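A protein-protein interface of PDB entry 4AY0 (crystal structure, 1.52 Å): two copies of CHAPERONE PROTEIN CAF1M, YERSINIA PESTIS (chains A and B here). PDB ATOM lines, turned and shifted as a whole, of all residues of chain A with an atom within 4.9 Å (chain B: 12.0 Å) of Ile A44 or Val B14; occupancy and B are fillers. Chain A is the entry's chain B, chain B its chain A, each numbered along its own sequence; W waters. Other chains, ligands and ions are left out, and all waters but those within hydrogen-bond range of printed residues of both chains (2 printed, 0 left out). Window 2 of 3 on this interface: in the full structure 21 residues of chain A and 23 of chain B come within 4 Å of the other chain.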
ATOM      1  N   VAL A  34     -13.949  -0.629  19.399  1.00  0.00           N
ATOM      2  CA  VAL A  34     -14.771  -1.051  18.264  1.00  0.00           C
ATOM      3  C   VAL A  34     -15.833  -2.027  18.756  1.00  0.00           C
ATOM      4  O   VAL A  34     -15.591  -2.823  19.665  1.00  0.00           O
ATOM      5  CB  VAL A  34     -13.950  -1.670  17.097  1.00  0.00           C
ATOM      6  CG1 VAL A  34     -12.984  -0.650  16.514  1.00  0.00           C
ATOM      7  CG2 VAL A  34     -13.203  -2.916  17.547  1.00  0.00           C
ATOM      8  N   LYS A  35     -17.028  -1.938  18.183  1.00  0.00           N
ATOM      9  CA  LYS A  35     -18.125  -2.796  18.590  1.00  0.00           C
ATOM     10  C   LYS A  35     -18.842  -3.390  17.385  1.00  0.00           C
ATOM     11  O   LYS A  35     -19.149  -2.684  16.417  1.00  0.00           O
ATOM     12  CB  LYS A  35     -19.111  -2.016  19.463  1.00  0.00           C
ATOM     13  CG  LYS A  35     -20.417  -2.754  19.750  1.00  0.00           C
ATOM     14  CD  LYS A  35     -21.275  -2.009  20.752  1.00  0.00           C
ATOM     15  N   ASN A  36     -19.090  -4.694  17.451  1.00  0.00           N
ATOM     16  CA  ASN A  36     -19.870  -5.404  16.448  1.00  0.00           C
ATOM     17  C   ASN A  36     -21.342  -5.307  16.839  1.00  0.00           C
ATOM     18  O   ASN A  36     -21.736  -5.781  17.903  1.00  0.00           O
ATOM     19  CB  ASN A  36     -19.404  -6.863  16.388  1.00  0.00           C
ATOM     20  CG  ASN A  36     -20.128  -7.683  15.326  1.00  0.00           C
ATOM     21  OD1 ASN A  36     -20.934  -7.162  14.556  1.00  0.00           O
ATOM     22  ND2 ASN A  36     -19.827  -8.976  15.279  1.00  0.00           N
ATOM     23  N   THR A  37     -22.151  -4.675  15.993  1.00  0.00           N
ATOM     24  CA  THR A  37     -23.562  -4.459  16.317  1.00  0.00           C
ATOM     25  C   THR A  37     -24.450  -5.631  15.915  1.00  0.00           C
ATOM     26  O   THR A  37     -25.630  -5.670  16.273  1.00  0.00           O
ATOM     27  CB  THR A  37     -24.113  -3.171  15.665  1.00  0.00           C
ATOM     28  OG1 THR A  37     -24.119  -3.316  14.239  1.00  0.00           O
ATOM     29  CG2 THR A  37     -23.268  -1.976  16.048  1.00  0.00           C
ATOM     30  N   VAL A  42     -17.555 -11.212  12.893  1.00  0.00           N
ATOM     31  CA  VAL A  42     -16.937 -10.568  11.741  1.00  0.00           C
ATOM     32  C   VAL A  42     -15.422 -10.524  11.905  1.00  0.00           C
ATOM     33  O   VAL A  42     -14.910 -10.273  12.999  1.00  0.00           O
ATOM     34  CB  VAL A  42     -17.486  -9.133  11.512  1.00  0.00           C
ATOM     35  CG1 VAL A  42     -18.955  -9.175  11.125  1.00  0.00           C
ATOM     36  CG2 VAL A  42     -17.290  -8.275  12.751  1.00  0.00           C
ATOM     37  N   LEU A  43     -14.704 -10.782  10.819  1.00  0.00           N
ATOM     38  CA  LEU A  43     -13.261 -10.592  10.822  1.00  0.00           C
ATOM     39  C   LEU A  43     -13.021  -9.137  10.466  1.00  0.00           C
ATOM     40  O   LEU A  43     -13.403  -8.691   9.383  1.00  0.00           O
ATOM     41  CB  LEU A  43     -12.600 -11.492   9.779  1.00  0.00           C
ATOM     42  CG  LEU A  43     -11.091 -11.301   9.606  1.00  0.00           C
ATOM     43  CD1 LEU A  43     -10.351 -11.738  10.858  1.00  0.00           C
ATOM     44  CD2 LEU A  43     -10.577 -12.039   8.380  1.00  0.00           C
ATOM     45  N   ILE A  44     -12.405  -8.376  11.362  1.00  0.00           N
ATOM     46  CA  ILE A  44     -12.137  -6.983  11.010  1.00  0.00           C
ATOM     47  C   ILE A  44     -10.672  -6.662  10.771  1.00  0.00           C
ATOM     48  O   ILE A  44      -9.784  -7.088  11.521  1.00  0.00           O
ATOM     49  CB  ILE A  44     -12.763  -5.958  11.974  1.00  0.00           C
ATOM     50  CG1 ILE A  44     -12.307  -6.200  13.405  1.00  0.00           C
ATOM     51  CG2 ILE A  44     -14.288  -5.956  11.871  1.00  0.00           C
ATOM     52  CD1 ILE A  44     -12.406  -4.953  14.231  1.00  0.00           C
ATOM     53  N   GLN A  45     -10.438  -5.921   9.691  1.00  0.00           N
ATOM     54  CA  GLN A  45      -9.115  -5.439   9.329  1.00  0.00           C
ATOM     55  C   GLN A  45      -9.123  -3.942   9.570  1.00  0.00           C
ATOM     56  O   GLN A  45      -9.967  -3.214   9.030  1.00  0.00           O
ATOM     57  CB  GLN A  45      -8.809  -5.729   7.854  1.00  0.00           C
ATOM     58  N   SER A  46      -8.197  -3.481  10.398  1.00  0.00           N
ATOM     59  CA  SER A  46      -8.118  -2.063  10.717  1.00  0.00           C
ATOM     60  C   SER A  46      -6.804  -1.484  10.216  1.00  0.00           C
ATOM     61  O   SER A  46      -5.726  -1.997  10.537  1.00  0.00           O
ATOM     62  CB  SER A  46      -8.256  -1.853  12.222  1.00  0.00           C
ATOM     63  OG  SER A  46      -9.424  -2.491  12.704  1.00  0.00           O
ATOM     64  N   PRO A  66      -4.171  -5.748  14.032  1.00  0.00           N
ATOM     65  CA  PRO A  66      -4.515  -5.266  12.695  1.00  0.00           C
ATOM     66  C   PRO A  66      -5.637  -6.074  12.062  1.00  0.00           C
ATOM     67  O   PRO A  66      -6.286  -5.598  11.128  1.00  0.00           O
ATOM     68  CB  PRO A  66      -3.210  -5.459  11.912  1.00  0.00           C
ATOM     69  CG  PRO A  66      -2.521  -6.594  12.608  1.00  0.00           C
ATOM     70  CD  PRO A  66      -2.838  -6.381  14.067  1.00  0.00           C
ATOM     71  N   LEU A  67      -5.867  -7.275  12.576  1.00  0.00           N
ATOM     72  CA  LEU A  67      -6.802  -8.218  11.977  1.00  0.00           C
ATOM     73  C   LEU A  67      -7.214  -9.189  13.077  1.00  0.00           C
ATOM     74  O   LEU A  67      -6.353  -9.833  13.672  1.00  0.00           O
ATOM     75  CB  LEU A  67      -6.095  -8.967  10.835  1.00  0.00           C
ATOM     76  CG  LEU A  67      -6.887  -9.884   9.899  1.00  0.00           C
ATOM     77  CD1 LEU A  67      -7.975  -9.118   9.162  1.00  0.00           C
ATOM     78  CD2 LEU A  67      -5.956 -10.587   8.909  1.00  0.00           C
ATOM     79  N   PHE A  68      -8.508  -9.272  13.377  1.00  0.00           N
ATOM     80  CA  PHE A  68      -8.985 -10.206  14.404  1.00  0.00           C
ATOM     81  C   PHE A  68     -10.477 -10.470  14.286  1.00  0.00           C
ATOM     82  O   PHE A  68     -11.204  -9.730  13.621  1.00  0.00           O
ATOM     83  CB  PHE A  68      -8.652  -9.701  15.818  1.00  0.00           C
ATOM     84  CG  PHE A  68      -9.520  -8.559  16.287  1.00  0.00           C
ATOM     85  CD1 PHE A  68      -9.283  -7.265  15.849  1.00  0.00           C
ATOM     86  CD2 PHE A  68     -10.584  -8.783  17.162  1.00  0.00           C
ATOM     87  CE1 PHE A  68     -10.072  -6.215  16.285  1.00  0.00           C
ATOM     88  CE2 PHE A  68     -11.388  -7.739  17.598  1.00  0.00           C
ATOM     89  CZ  PHE A  68     -11.131  -6.446  17.158  1.00  0.00           C
ATOM     90  N   LEU A  70     -14.066 -10.480  15.713  1.00  0.00           N
ATOM     91  CA  LEU A  70     -14.915  -9.826  16.700  1.00  0.00           C
ATOM     92  C   LEU A  70     -16.253 -10.556  16.700  1.00  0.00           C
ATOM     93  O   LEU A  70     -16.993 -10.502  15.714  1.00  0.00           O
ATOM     94  CB  LEU A  70     -15.095  -8.355  16.318  1.00  0.00           C
ATOM     95  CG  LEU A  70     -15.764  -7.357  17.263  1.00  0.00           C
ATOM     96  CD1 LEU A  70     -14.971  -7.185  18.545  1.00  0.00           C
ATOM     97  CD2 LEU A  70     -15.929  -6.021  16.553  1.00  0.00           C
ATOM     98  N   LEU A  78      -8.672  -1.246  20.120  1.00  0.00           N
ATOM     99  CA  LEU A  78      -7.529  -1.219  19.201  1.00  0.00           C
ATOM    100  C   LEU A  78      -6.504  -0.229  19.725  1.00  0.00           C
ATOM    101  O   LEU A  78      -6.864   0.839  20.220  1.00  0.00           O
ATOM    102  CB  LEU A  78      -7.954  -0.719  17.819  1.00  0.00           C
ATOM    103  CG  LEU A  78      -9.120  -1.335  17.050  1.00  0.00           C
ATOM    104  CD1 LEU A  78      -9.389  -0.521  15.797  1.00  0.00           C
ATOM    105  CD2 LEU A  78      -8.820  -2.770  16.689  1.00  0.00           C
ATOM    106  N   VAL A  99     -12.048   0.578   9.169  1.00  0.00           N
ATOM    107  CA  VAL A  99     -12.237  -0.765   9.688  1.00  0.00           C
ATOM    108  C   VAL A  99     -13.114  -1.509   8.700  1.00  0.00           C
ATOM    109  O   VAL A  99     -14.260  -1.112   8.460  1.00  0.00           O
ATOM    110  CB  VAL A  99     -12.852  -0.736  11.098  1.00  0.00           C
ATOM    111  CG1 VAL A  99     -13.148  -2.141  11.585  1.00  0.00           C
ATOM    112  CG2 VAL A  99     -11.895  -0.031  12.067  1.00  0.00           C
ATOM    113  N   LYS A 100     -12.552  -2.558   8.100  1.00  0.00           N
ATOM    114  CA  LYS A 100     -13.226  -3.319   7.056  1.00  0.00           C
ATOM    115  C   LYS A 100     -13.532  -4.705   7.572  1.00  0.00           C
ATOM    116  O   LYS A 100     -12.635  -5.408   8.046  1.00  0.00           O
ATOM    117  CB  LYS A 100     -12.351  -3.415   5.804  1.00  0.00           C
ATOM    118  N   GLY A 101     -14.798  -5.101   7.488  1.00  0.00           N
ATOM    119  CA  GLY A 101     -15.216  -6.387   8.012  1.00  0.00           C
ATOM    120  C   GLY A 101     -15.734  -7.329   6.945  1.00  0.00           C
ATOM    121  O   GLY A 101     -16.378  -6.899   5.985  1.00  0.00           O
ATOM    122  N   ASN A 119     -16.060   1.050   7.585  1.00  0.00           N
ATOM    123  CA  ASN A 119     -16.305   2.260   8.357  1.00  0.00           C
ATOM    124  C   ASN A 119     -15.011   3.052   8.483  1.00  0.00           C
ATOM    125  O   ASN A 119     -14.042   2.565   9.064  1.00  0.00           O
ATOM    126  CB  ASN A 119     -16.838   1.875   9.741  1.00  0.00           C
ATOM    127  CG  ASN A 119     -17.139   3.077  10.623  1.00  0.00           C
ATOM    128  OD1 ASN A 119     -16.962   4.229  10.223  1.00  0.00           O
ATOM    129  ND2 ASN A 119     -17.609   2.805  11.834  1.00  0.00           N
ATOM    130  N   GLY B  13     -22.606  -1.625  11.469  1.00  0.00           N
ATOM    131  CA  GLY B  13     -22.028  -2.948  11.614  1.00  0.00           C
ATOM    132  C   GLY B  13     -20.936  -2.949  12.665  1.00  0.00           C
ATOM    133  O   GLY B  13     -21.080  -3.568  13.724  1.00  0.00           O
ATOM    134  N   VAL B  14     -19.841  -2.258  12.366  1.00  0.00           N
ATOM    135  CA  VAL B  14     -18.775  -2.058  13.341  1.00  0.00           C
ATOM    136  C   VAL B  14     -18.664  -0.575  13.678  1.00  0.00           C
ATOM    137  O   VAL B  14     -18.269   0.237  12.838  1.00  0.00           O
ATOM    138  CB  VAL B  14     -17.416  -2.594  12.851  1.00  0.00           C
ATOM    139  CG1 VAL B  14     -16.306  -2.148  13.789  1.00  0.00           C
ATOM    140  CG2 VAL B  14     -17.455  -4.111  12.773  1.00  0.00           C
ATOM    141  N   THR B  15     -19.018  -0.232  14.909  1.00  0.00           N
ATOM    142  CA  THR B  15     -18.969   1.158  15.356  1.00  0.00           C
ATOM    143  C   THR B  15     -17.619   1.448  15.991  1.00  0.00           C
ATOM    144  O   THR B  15     -17.083   0.621  16.732  1.00  0.00           O
ATOM    145  CB  THR B  15     -20.063   1.458  16.380  1.00  0.00           C
ATOM    146  OG1 THR B  15     -19.791   0.745  17.594  1.00  0.00           O
ATOM    147  CG2 THR B  15     -21.412   1.047  15.841  1.00  0.00           C
ATOM    148  N   ILE B  16     -17.076   2.624  15.694  1.00  0.00           N
ATOM    149  CA  ILE B  16     -15.789   3.044  16.225  1.00  0.00           C
ATOM    150  C   ILE B  16     -16.028   4.180  17.222  1.00  0.00           C
ATOM    151  O   ILE B  16     -16.651   5.194  16.882  1.00  0.00           O
ATOM    152  CB  ILE B  16     -14.851   3.523  15.097  1.00  0.00           C
ATOM    153  CG1 ILE B  16     -14.718   2.451  14.008  1.00  0.00           C
ATOM    154  CG2 ILE B  16     -13.486   3.881  15.655  1.00  0.00           C
ATOM    155  CD1 ILE B  16     -14.056   2.944  12.736  1.00  0.00           C
ATOM    156  N   GLY B  17     -15.541   4.013  18.451  1.00  0.00           N
ATOM    157  CA  GLY B  17     -15.777   5.003  19.495  1.00  0.00           C
ATOM    158  C   GLY B  17     -17.225   5.031  19.938  1.00  0.00           C
ATOM    159  O   GLY B  17     -18.021   4.165  19.570  1.00  0.00           O
ATOM    160  N   GLU B  18     -17.579   6.034  20.728  1.00  0.00           N
ATOM    161  CA  GLU B  18     -18.938   6.122  21.231  1.00  0.00           C
ATOM    162  C   GLU B  18     -19.318   7.571  21.447  1.00  0.00           C
ATOM    163  O   GLU B  18     -18.890   8.196  22.420  1.00  0.00           O
ATOM    164  CB  GLU B  18     -19.070   5.341  22.540  1.00  0.00           C
ATOM    165  CG  GLU B  18     -20.480   5.340  23.083  1.00  0.00           C
ATOM    166  CD  GLU B  18     -20.576   4.680  24.439  1.00  0.00           C
ATOM    167  OE1 GLU B  18     -20.299   3.467  24.540  1.00  0.00           O
ATOM    168  OE2 GLU B  18     -20.936   5.377  25.401  1.00  0.00           O
ATOM    169  N   SER B  19     -20.104   8.120  20.528  1.00  0.00           N
ATOM    170  CA  SER B  19     -20.502   9.510  20.642  1.00  0.00           C
ATOM    171  C   SER B  19     -21.400   9.749  21.855  1.00  0.00           C
ATOM    172  O   SER B  19     -22.139   8.856  22.295  1.00  0.00           O
ATOM    173  CB  SER B  19     -21.199   9.971  19.362  1.00  0.00           C
ATOM    174  OG  SER B  19     -20.299   9.887  18.273  1.00  0.00           O
ATOM    175  N   THR B  37     -27.744   4.572   7.142  1.00  0.00           N
ATOM    176  CA  THR B  37     -26.712   3.806   6.449  1.00  0.00           C
ATOM    177  C   THR B  37     -27.276   2.768   5.478  1.00  0.00           C
ATOM    178  O   THR B  37     -26.522   2.143   4.737  1.00  0.00           O
ATOM    179  CB  THR B  37     -25.762   3.107   7.446  1.00  0.00           C
ATOM    180  OG1 THR B  37     -26.500   2.157   8.229  1.00  0.00           O
ATOM    181  CG2 THR B  37     -25.119   4.136   8.372  1.00  0.00           C
ATOM    182  N   ASN B 119     -31.312   3.167  18.299  1.00  0.00           N
ATOM    183  CA  ASN B 119     -30.017   3.715  18.681  1.00  0.00           C
ATOM    184  C   ASN B 119     -30.178   4.805  19.731  1.00  0.00           C
ATOM    185  O   ASN B 119     -30.918   5.767  19.517  1.00  0.00           O
ATOM    186  CB  ASN B 119     -29.313   4.282  17.447  1.00  0.00           C
ATOM    187  CG  ASN B 119     -27.861   4.618  17.706  1.00  0.00           C
ATOM    188  OD1 ASN B 119     -27.406   4.630  18.852  1.00  0.00           O
ATOM    189  ND2 ASN B 119     -27.123   4.902  16.639  1.00  0.00           N
HETATM  190  O   HOH W   1     -21.719  -6.223  12.300  1.00  0.00           O
HETATM  191  O   HOH W   2     -18.617   4.483  14.113  1.00  0.00           O
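Among the printed residues, pairs that only touch across the chains: Lys A35 with Val B14 (3.2 Å), Val A34 with Thr B15 (3.2 Å), Asn A36 with Gly B13 (3.5 Å), Thr A37 with Thr B15 (3.6 Å), Asn A119 with Ile B16 (3.6 Å), Val A99 with Ile B16 (3.7 Å), Ile A44 with Val B14 (3.8 Å) and Val A99 with Val B14 (3.9 Å).
Positions printed for both chains: 37 and 119.
Of the 12 pairs that touch across the chains among the printed residues, none has its exchanged pair printed and touching as well.
O of Val B14 is in hydrogen-bond range of ND2 of Asn A119.
The backbone carbonyl oxygen of Lys A35 lies close to the backbone carbonyl oxygen of Gly B13 (3.4 Å).
The backbone carbonyl oxygen (O) of Gly B13 sits at hydrogen-bond distance from the backbone NH (N) of Thr A37.
N of Thr B15 is in hydrogen-bond range of O of Lys A35 (2.9 Å).
Water W1 lies within hydrogen-bond range of the side-chain amide oxygen of Asn A36 (2.6 Å) and the backbone carbonyl oxygen of Gly B13 (3.1 Å).
Water W2 bridges the backbone NH of Ile B16 (2.9 Å) and the side-chain amide nitrogen of Asn A119 (3.0 Å).
Val A34 touches just one residue of chain B: Thr B15.
Printed residues of chain B within 4 Å of Asn A36: Gly B13.
No residue of chain B comes within 4 Å of Leu A43.
Ile A44 touches one residue of chain B.
No residue of chain B comes within 4 Å of Gln A45.
No residue of chain B comes within 4 Å of Ser A46.
No residue of chain B comes within 4 Å of Leu A67.
No residue of chain B comes within 4 Å of Phe A68.
No residue of chain B comes within 4 Å of Leu A70.
Leu A78 touches none of the printed residues of chain B.
No residue of chain B comes within 4 Å of Lys A100.
No residue of chain B comes within 4 Å of Gly A101.
Asn A119 touches two residues of chain B.
Val B14 touches just these residues of chain A: Lys A35 (3.2 Å), Ile A44 (3.8 Å), Val A99 (3.9 Å) and Asn A119 (2.8 Å).
Of the printed residues of chain A, Thr B15 touches Val A34 (3.2 Å), Lys A35 (2.9 Å) and Thr A37 (3.6 Å).
Of the printed residues of chain A, Ile B16 touches Val A99 and Asn A119.
The backbone carbonyl oxygen (O) of Phe A68 sits at hydrogen-bond distance from the backbone NH (N) of Ile A44.
The backbone carbonyl oxygen (O) of Asn A119 is in hydrogen-bond range of the backbone NH (N) of Val A99 (2.8 Å).
The side-chain amide nitrogen (ND2) of Asn A36 sits at hydrogen-bond distance from the backbone carbonyl oxygen (O) of Leu A70 (3.2 Å).
Hydrophobic or aromatic side chains of chain B that line the printed part of chain A: Val B14 and Ile B16.
Among the printed residues, 12 pairs touch across the chains.
Among the printed residues, no Asp or Glu carboxylate lies within 4 Å of a Lys or Arg side-chain nitrogen of the other chain.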
